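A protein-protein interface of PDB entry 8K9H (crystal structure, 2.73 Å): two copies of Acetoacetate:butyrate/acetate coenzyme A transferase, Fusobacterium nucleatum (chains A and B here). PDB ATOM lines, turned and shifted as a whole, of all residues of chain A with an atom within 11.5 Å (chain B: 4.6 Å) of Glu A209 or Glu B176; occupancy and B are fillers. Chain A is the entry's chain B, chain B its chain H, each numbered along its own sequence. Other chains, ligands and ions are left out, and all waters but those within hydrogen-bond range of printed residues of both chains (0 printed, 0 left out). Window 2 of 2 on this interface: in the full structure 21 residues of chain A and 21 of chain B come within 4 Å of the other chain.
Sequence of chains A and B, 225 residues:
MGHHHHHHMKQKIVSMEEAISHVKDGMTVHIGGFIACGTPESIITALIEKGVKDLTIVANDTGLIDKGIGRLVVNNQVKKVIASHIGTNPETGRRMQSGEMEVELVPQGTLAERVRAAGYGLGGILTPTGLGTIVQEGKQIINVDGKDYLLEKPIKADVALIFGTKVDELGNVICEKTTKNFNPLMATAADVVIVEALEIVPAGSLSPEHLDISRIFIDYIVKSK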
ATOM      1  N   ASP A 168       9.117   1.839  30.471  1.00  0.00           N
ATOM      2  CA  ASP A 168       8.822   0.432  30.238  1.00  0.00           C
ATOM      3  C   ASP A 168       9.133  -0.379  31.498  1.00  0.00           C
ATOM      4  O   ASP A 168       9.796   0.093  32.424  1.00  0.00           O
ATOM      5  CB  ASP A 168       9.541  -0.083  28.970  1.00  0.00           C
ATOM      6  CG  ASP A 168      10.944  -0.667  29.212  1.00  0.00           C
ATOM      7  OD1 ASP A 168      11.518  -0.591  30.322  1.00  0.00           O
ATOM      8  OD2 ASP A 168      11.488  -1.216  28.227  1.00  0.00           O
ATOM      9  N   ASN A 172      13.423   1.431  31.634  1.00  0.00           N
ATOM     10  CA  ASN A 172      13.745   2.424  30.606  1.00  0.00           C
ATOM     11  C   ASN A 172      12.732   3.566  30.649  1.00  0.00           C
ATOM     12  O   ASN A 172      11.524   3.336  30.762  1.00  0.00           O
ATOM     13  CB  ASN A 172      13.751   1.788  29.208  1.00  0.00           C
ATOM     14  CG  ASN A 172      14.833   0.711  29.039  1.00  0.00           C
ATOM     15  OD1 ASN A 172      16.030   0.947  29.285  1.00  0.00           O
ATOM     16  ND2 ASN A 172      14.414  -0.479  28.606  1.00  0.00           N
ATOM     17  N   VAL A 173      13.220   4.802  30.564  1.00  0.00           N
ATOM     18  CA  VAL A 173      12.378   5.982  30.737  1.00  0.00           C
ATOM     19  C   VAL A 173      12.454   6.848  29.492  1.00  0.00           C
ATOM     20  O   VAL A 173      13.507   6.930  28.847  1.00  0.00           O
ATOM     21  CB  VAL A 173      12.776   6.818  31.969  1.00  0.00           C
ATOM     22  CG1 VAL A 173      11.841   8.013  32.100  1.00  0.00           C
ATOM     23  CG2 VAL A 173      12.766   5.957  33.236  1.00  0.00           C
ATOM     24  N   ILE A 174      11.327   7.486  29.152  1.00  0.00           N
ATOM     25  CA  ILE A 174      11.237   8.486  28.091  1.00  0.00           C
ATOM     26  C   ILE A 174      10.689   9.761  28.707  1.00  0.00           C
ATOM     27  O   ILE A 174       9.597   9.753  29.294  1.00  0.00           O
ATOM     28  CB  ILE A 174      10.348   8.028  26.926  1.00  0.00           C
ATOM     29  CG1 ILE A 174      11.032   6.918  26.134  1.00  0.00           C
ATOM     30  CG2 ILE A 174      10.020   9.199  26.012  1.00  0.00           C
ATOM     31  CD1 ILE A 174      10.529   6.782  24.709  1.00  0.00           C
ATOM     32  N   CYS A 175      11.451  10.855  28.588  1.00  0.00           N
ATOM     33  CA  CYS A 175      11.025  12.181  29.032  1.00  0.00           C
ATOM     34  C   CYS A 175      10.803  13.030  27.790  1.00  0.00           C
ATOM     35  O   CYS A 175      11.767  13.465  27.152  1.00  0.00           O
ATOM     36  CB  CYS A 175      12.053  12.832  29.954  1.00  0.00           C
ATOM     37  SG  CYS A 175      12.607  11.819  31.355  1.00  0.00           S
ATOM     38  N   LYS A 180      12.684  16.745  30.105  1.00  0.00           N
ATOM     39  CA  LYS A 180      13.972  16.110  30.298  1.00  0.00           C
ATOM     40  C   LYS A 180      14.759  16.801  31.404  1.00  0.00           C
ATOM     41  O   LYS A 180      15.046  16.185  32.432  1.00  0.00           O
ATOM     42  CB  LYS A 180      14.725  16.099  28.975  1.00  0.00           C
ATOM     43  CG  LYS A 180      14.282  14.967  28.091  1.00  0.00           C
ATOM     44  CD  LYS A 180      15.037  14.977  26.783  1.00  0.00           C
ATOM     45  CE  LYS A 180      14.216  15.611  25.712  1.00  0.00           C
ATOM     46  NZ  LYS A 180      12.899  14.934  25.662  1.00  0.00           N
ATOM     47  N   GLY A 204      10.374  -3.592  26.616  1.00  0.00           N
ATOM     48  CA  GLY A 204      10.747  -3.683  25.221  1.00  0.00           C
ATOM     49  C   GLY A 204       9.875  -2.876  24.285  1.00  0.00           C
ATOM     50  O   GLY A 204      10.239  -2.716  23.111  1.00  0.00           O
ATOM     51  N   SER A 205       8.734  -2.361  24.765  1.00  0.00           N
ATOM     52  CA  SER A 205       7.838  -1.573  23.922  1.00  0.00           C
ATOM     53  C   SER A 205       8.531  -0.350  23.328  1.00  0.00           C
ATOM     54  O   SER A 205       8.104   0.143  22.275  1.00  0.00           O
ATOM     55  CB  SER A 205       6.602  -1.158  24.740  1.00  0.00           C
ATOM     56  OG  SER A 205       6.068   0.113  24.374  1.00  0.00           O
ATOM     57  N   LEU A 206       9.600   0.129  23.967  1.00  0.00           N
ATOM     58  CA  LEU A 206      10.275   1.361  23.595  1.00  0.00           C
ATOM     59  C   LEU A 206      11.568   1.048  22.858  1.00  0.00           C
ATOM     60  O   LEU A 206      12.285   0.104  23.210  1.00  0.00           O
ATOM     61  CB  LEU A 206      10.557   2.205  24.834  1.00  0.00           C
ATOM     62  CG  LEU A 206       9.285   2.555  25.607  1.00  0.00           C
ATOM     63  CD1 LEU A 206       9.610   3.396  26.833  1.00  0.00           C
ATOM     64  CD2 LEU A 206       8.283   3.268  24.716  1.00  0.00           C
ATOM     65  N   SER A 207      11.855   1.856  21.840  1.00  0.00           N
ATOM     66  CA  SER A 207      12.976   1.601  20.950  1.00  0.00           C
ATOM     67  C   SER A 207      14.302   1.878  21.656  1.00  0.00           C
ATOM     68  O   SER A 207      14.415   2.840  22.422  1.00  0.00           O
ATOM     69  CB  SER A 207      12.854   2.485  19.708  1.00  0.00           C
ATOM     70  OG  SER A 207      13.997   2.403  18.879  1.00  0.00           O
ATOM     71  N   PRO A 208      15.335   1.077  21.395  1.00  0.00           N
ATOM     72  CA  PRO A 208      16.671   1.389  21.936  1.00  0.00           C
ATOM     73  C   PRO A 208      17.213   2.742  21.498  1.00  0.00           C
ATOM     74  O   PRO A 208      18.206   3.208  22.077  1.00  0.00           O
ATOM     75  CB  PRO A 208      17.555   0.256  21.397  1.00  0.00           C
ATOM     76  CG  PRO A 208      16.637  -0.754  20.900  1.00  0.00           C
ATOM     77  CD  PRO A 208      15.349  -0.098  20.524  1.00  0.00           C
ATOM     78  N   GLU A 209      16.597   3.381  20.504  1.00  0.00           N
ATOM     79  CA  GLU A 209      17.077   4.640  19.958  1.00  0.00           C
ATOM     80  C   GLU A 209      16.337   5.853  20.497  1.00  0.00           C
ATOM     81  O   GLU A 209      16.815   6.974  20.313  1.00  0.00           O
ATOM     82  CB  GLU A 209      16.961   4.619  18.431  1.00  0.00           C
ATOM     83  CG  GLU A 209      17.617   3.427  17.810  1.00  0.00           C
ATOM     84  CD  GLU A 209      18.988   3.748  17.302  1.00  0.00           C
ATOM     85  OE1 GLU A 209      19.589   2.889  16.610  1.00  0.00           O
ATOM     86  OE2 GLU A 209      19.463   4.871  17.590  1.00  0.00           O
ATOM     87  N   HIS A 210      15.197   5.657  21.159  1.00  0.00           N
ATOM     88  CA  HIS A 210      14.313   6.752  21.531  1.00  0.00           C
ATOM     89  C   HIS A 210      14.268   6.964  23.032  1.00  0.00           C
ATOM     90  O   HIS A 210      13.323   7.580  23.538  1.00  0.00           O
ATOM     91  CB  HIS A 210      12.888   6.516  21.020  1.00  0.00           C
ATOM     92  CG  HIS A 210      12.795   6.209  19.555  1.00  0.00           C
ATOM     93  ND1 HIS A 210      11.755   5.478  19.018  1.00  0.00           N
ATOM     94  CD2 HIS A 210      13.600   6.538  18.515  1.00  0.00           C
ATOM     95  CE1 HIS A 210      11.932   5.360  17.714  1.00  0.00           C
ATOM     96  NE2 HIS A 210      13.042   5.996  17.382  1.00  0.00           N
ATOM     97  N   LEU A 211      15.253   6.461  23.755  1.00  0.00           N
ATOM     98  CA  LEU A 211      15.175   6.469  25.205  1.00  0.00           C
ATOM     99  C   LEU A 211      15.974   7.629  25.791  1.00  0.00           C
ATOM    100  O   LEU A 211      16.914   8.148  25.181  1.00  0.00           O
ATOM    101  CB  LEU A 211      15.675   5.147  25.776  1.00  0.00           C
ATOM    102  CG  LEU A 211      14.872   3.879  25.573  1.00  0.00           C
ATOM    103  CD1 LEU A 211      15.710   2.716  26.055  1.00  0.00           C
ATOM    104  CD2 LEU A 211      13.546   3.962  26.309  1.00  0.00           C
ATOM    105  N   ASP A 212      15.575   8.045  26.980  1.00  0.00           N
ATOM    106  CA  ASP A 212      16.269   9.109  27.684  1.00  0.00           C
ATOM    107  C   ASP A 212      17.034   8.628  28.911  1.00  0.00           C
ATOM    108  O   ASP A 212      18.033   9.253  29.292  1.00  0.00           O
ATOM    109  CB  ASP A 212      15.266  10.191  28.093  1.00  0.00           C
ATOM    110  CG  ASP A 212      14.739  10.968  26.901  1.00  0.00           C
ATOM    111  OD1 ASP A 212      15.573  11.544  26.152  1.00  0.00           O
ATOM    112  OD2 ASP A 212      13.499  10.996  26.709  1.00  0.00           O
ATOM    113  N   ILE A 213      16.598   7.525  29.526  1.00  0.00           N
ATOM    114  CA  ILE A 213      17.214   6.972  30.725  1.00  0.00           C
ATOM    115  C   ILE A 213      17.173   5.451  30.612  1.00  0.00           C
ATOM    116  O   ILE A 213      16.089   4.870  30.491  1.00  0.00           O
ATOM    117  CB  ILE A 213      16.495   7.426  32.006  1.00  0.00           C
ATOM    118  CG1 ILE A 213      16.339   8.950  32.041  1.00  0.00           C
ATOM    119  CG2 ILE A 213      17.255   6.952  33.211  1.00  0.00           C
ATOM    120  CD1 ILE A 213      15.422   9.464  33.131  1.00  0.00           C
ATOM    121  N   SER A 214      18.344   4.808  30.656  1.00  0.00           N
ATOM    122  CA  SER A 214      18.433   3.354  30.629  1.00  0.00           C
ATOM    123  C   SER A 214      17.869   2.728  31.904  1.00  0.00           C
ATOM    124  O   SER A 214      17.797   3.346  32.969  1.00  0.00           O
ATOM    125  CB  SER A 214      19.879   2.892  30.467  1.00  0.00           C
ATOM    126  OG  SER A 214      19.951   1.476  30.533  1.00  0.00           O
ATOM    127  N   ARG A 215      17.492   1.453  31.779  1.00  0.00           N
ATOM    128  CA  ARG A 215      16.904   0.698  32.886  1.00  0.00           C
ATOM    129  C   ARG A 215      17.874   0.516  34.042  1.00  0.00           C
ATOM    130  O   ARG A 215      17.446   0.435  35.197  1.00  0.00           O
ATOM    131  CB  ARG A 215      16.457  -0.677  32.387  1.00  0.00           C
ATOM    132  CG  ARG A 215      17.608  -1.419  31.729  1.00  0.00           C
ATOM    133  CD  ARG A 215      17.252  -2.817  31.345  1.00  0.00           C
ATOM    134  NE  ARG A 215      16.863  -3.592  32.510  1.00  0.00           N
ATOM    135  CZ  ARG A 215      16.737  -4.910  32.499  1.00  0.00           C
ATOM    136  NH1 ARG A 215      16.979  -5.580  31.374  1.00  0.00           N
ATOM    137  NH2 ARG A 215      16.370  -5.549  33.609  1.00  0.00           N
ATOM    138  N   THR B 165      23.543   8.093   9.844  1.00  0.00           N
ATOM    139  CA  THR B 165      22.746   7.214   9.002  1.00  0.00           C
ATOM    140  C   THR B 165      21.540   7.937   8.403  1.00  0.00           C
ATOM    141  O   THR B 165      21.006   7.486   7.384  1.00  0.00           O
ATOM    142  CB  THR B 165      22.305   5.953   9.772  1.00  0.00           C
ATOM    143  OG1 THR B 165      21.576   6.314  10.941  1.00  0.00           O
ATOM    144  CG2 THR B 165      23.501   5.116  10.182  1.00  0.00           C
ATOM    145  N   LYS B 166      21.137   9.066   8.984  1.00  0.00           N
ATOM    146  CA  LYS B 166      20.033   9.881   8.476  1.00  0.00           C
ATOM    147  C   LYS B 166      20.302  11.332   8.866  1.00  0.00           C
ATOM    148  O   LYS B 166      20.273  11.662  10.049  1.00  0.00           O
ATOM    149  CB  LYS B 166      18.702   9.426   9.057  1.00  0.00           C
ATOM    150  CG  LYS B 166      17.979   8.312   8.311  1.00  0.00           C
ATOM    151  CD  LYS B 166      16.526   8.275   8.800  1.00  0.00           C
ATOM    152  CE  LYS B 166      15.738   7.078   8.310  1.00  0.00           C
ATOM    153  NZ  LYS B 166      14.386   7.062   8.972  1.00  0.00           N
ATOM    154  N   ILE B 174      20.976  11.691  12.766  1.00  0.00           N
ATOM    155  CA  ILE B 174      20.709  10.469  13.504  1.00  0.00           C
ATOM    156  C   ILE B 174      21.823   9.485  13.188  1.00  0.00           C
ATOM    157  O   ILE B 174      22.156   9.280  12.016  1.00  0.00           O
ATOM    158  CB  ILE B 174      19.343   9.872  13.144  1.00  0.00           C
ATOM    159  CG1 ILE B 174      18.214  10.680  13.762  1.00  0.00           C
ATOM    160  CG2 ILE B 174      19.277   8.430  13.604  1.00  0.00           C
ATOM    161  CD1 ILE B 174      16.884  10.034  13.586  1.00  0.00           C
ATOM    162  N   CYS B 175      22.423   8.914  14.235  1.00  0.00           N
ATOM    163  CA  CYS B 175      23.376   7.812  14.134  1.00  0.00           C
ATOM    164  C   CYS B 175      22.729   6.586  14.766  1.00  0.00           C
ATOM    165  O   CYS B 175      22.405   6.596  15.957  1.00  0.00           O
ATOM    166  CB  CYS B 175      24.701   8.150  14.837  1.00  0.00           C
ATOM    167  SG  CYS B 175      25.299   9.883  14.684  1.00  0.00           S
ATOM    168  N   GLU B 176      22.495   5.550  13.978  1.00  0.00           N
ATOM    169  CA  GLU B 176      21.727   4.419  14.477  1.00  0.00           C
ATOM    170  C   GLU B 176      22.638   3.371  15.102  1.00  0.00           C
ATOM    171  O   GLU B 176      23.813   3.244  14.734  1.00  0.00           O
ATOM    172  CB  GLU B 176      20.892   3.789  13.357  1.00  0.00           C
ATOM    173  CG  GLU B 176      19.733   4.654  12.901  1.00  0.00           C
ATOM    174  CD  GLU B 176      18.842   3.957  11.873  1.00  0.00           C
ATOM    175  OE1 GLU B 176      19.195   2.827  11.438  1.00  0.00           O
ATOM    176  OE2 GLU B 176      17.794   4.552  11.504  1.00  0.00           O
ATOM    177  N   LYS B 177      22.080   2.624  16.066  1.00  0.00           N
ATOM    178  CA  LYS B 177      22.760   1.493  16.730  1.00  0.00           C
ATOM    179  C   LYS B 177      24.100   1.986  17.283  1.00  0.00           C
ATOM    180  O   LYS B 177      24.138   2.994  17.999  1.00  0.00           O
ATOM    181  CB  LYS B 177      22.848   0.320  15.765  1.00  0.00           C
ATOM    182  CG  LYS B 177      21.515  -0.323  15.451  1.00  0.00           C
ATOM    183  CD  LYS B 177      21.325  -0.458  13.954  1.00  0.00           C
ATOM    184  CE  LYS B 177      19.940  -0.973  13.618  1.00  0.00           C
ATOM    185  NZ  LYS B 177      19.956  -1.799  12.376  1.00  0.00           N
ATOM    186  N   THR B 178      25.214   1.332  16.985  1.00  0.00           N
ATOM    187  CA  THR B 178      26.489   1.733  17.558  1.00  0.00           C
ATOM    188  C   THR B 178      27.292   2.662  16.651  1.00  0.00           C
ATOM    189  O   THR B 178      28.525   2.574  16.639  1.00  0.00           O
ATOM    190  CB  THR B 178      27.314   0.492  17.927  1.00  0.00           C
ATOM    191  OG1 THR B 178      27.638  -0.275  16.753  1.00  0.00           O
ATOM    192  CG2 THR B 178      26.540  -0.382  18.911  1.00  0.00           C
ATOM    193  N   THR B 179      26.647   3.553  15.892  1.00  0.00           N
ATOM    194  CA  THR B 179      27.398   4.483  15.046  1.00  0.00           C
ATOM    195  C   THR B 179      27.541   5.861  15.669  1.00  0.00           C
ATOM    196  O   THR B 179      28.234   6.705  15.111  1.00  0.00           O
ATOM    197  CB  THR B 179      26.773   4.617  13.640  1.00  0.00           C
ATOM    198  OG1 THR B 179      25.393   4.990  13.737  1.00  0.00           O
ATOM    199  CG2 THR B 179      26.891   3.312  12.875  1.00  0.00           C
ATOM    200  N   LYS B 180      26.892   6.113  16.799  1.00  0.00           N
ATOM    201  CA  LYS B 180      27.176   7.282  17.632  1.00  0.00           C
ATOM    202  C   LYS B 180      28.385   6.930  18.489  1.00  0.00           C
ATOM    203  O   LYS B 180      28.268   6.372  19.580  1.00  0.00           O
ATOM    204  CB  LYS B 180      25.961   7.614  18.489  1.00  0.00           C
ATOM    205  CG  LYS B 180      25.273   6.381  19.045  1.00  0.00           C
ATOM    206  CD  LYS B 180      23.964   6.676  19.809  1.00  0.00           C
ATOM    207  CE  LYS B 180      22.717   6.254  19.059  1.00  0.00           C
ATOM    208  NZ  LYS B 180      22.798   4.848  18.587  1.00  0.00           N
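3 positions are printed for both chains. Of the 4 pairs that touch across the chains among the printed residues, none has its exchanged pair printed and touching as well.
Printed residues of chain B that touch a printed residue of chain A: Cys B175, Glu B176, Lys B177 and Lys B180. Of the 18 printed residues of chain A, 1 touches a printed residue of chain B. Among the printed residues, 4 pairs touch across the chains. Among the printed residues, Asp or Glu carboxylates within 4 Å of a Lys or Arg side-chain nitrogen of the other chain: Glu A209 with Lys B180.
The side-chain carboxylate (OE2) of Glu A209 lies within salt-bridge range of the side-chain amino group (NZ) of Lys B180 (3.5 Å). The side-chain carboxylate (OE1) of Glu A209 is in hydrogen-bond range of the backbone NH (N) of Lys B177 (2.6 Å).
OG1 of Thr B165 lies close to N of Glu B176, 3.3 Å away. The backbone carbonyl oxygen (O) of Glu B176 lies within hydrogen-bond range of the side-chain hydroxyl (OG1) of Thr B179, at 2.6 Å. OG of Ser A207 sits close to N of Glu A209, 3.2 Å away. NZ of Lys B180 lies close to O of Cys B175 (3.2 Å).
Pro A208 touches none of the printed residues of chain B. Glu A209 touches just these residues of chain B: Cys B175 (3.8 Å), Glu B176 (3.4 Å), Lys B177 (2.6 Å) and Lys B180 (3.5 Å). Ile A213 touches none of the printed residues of chain B. No residue of chain A comes within 4 Å of Ile B174. Of chain A, only Glu A209 (3.8 Å) comes within 4 Å of Cys B175. Glu B176 touches one residue of chain A. Lys B177 touches just one residue of chain A: Glu A209. Thr B178 touches none of the printed residues of chain A. Of chain A, only Glu A209 comes within 4 Å of Lys B180. The nearest printed residue of chain B that does not touch Glu A209 is Ile B174 (5.3 Å).
Among the printed residues, pairs that only touch across the chains: Glu A209 with Cys B175 (3.8 Å) and Glu A209 with Glu B176 (3.4 Å).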
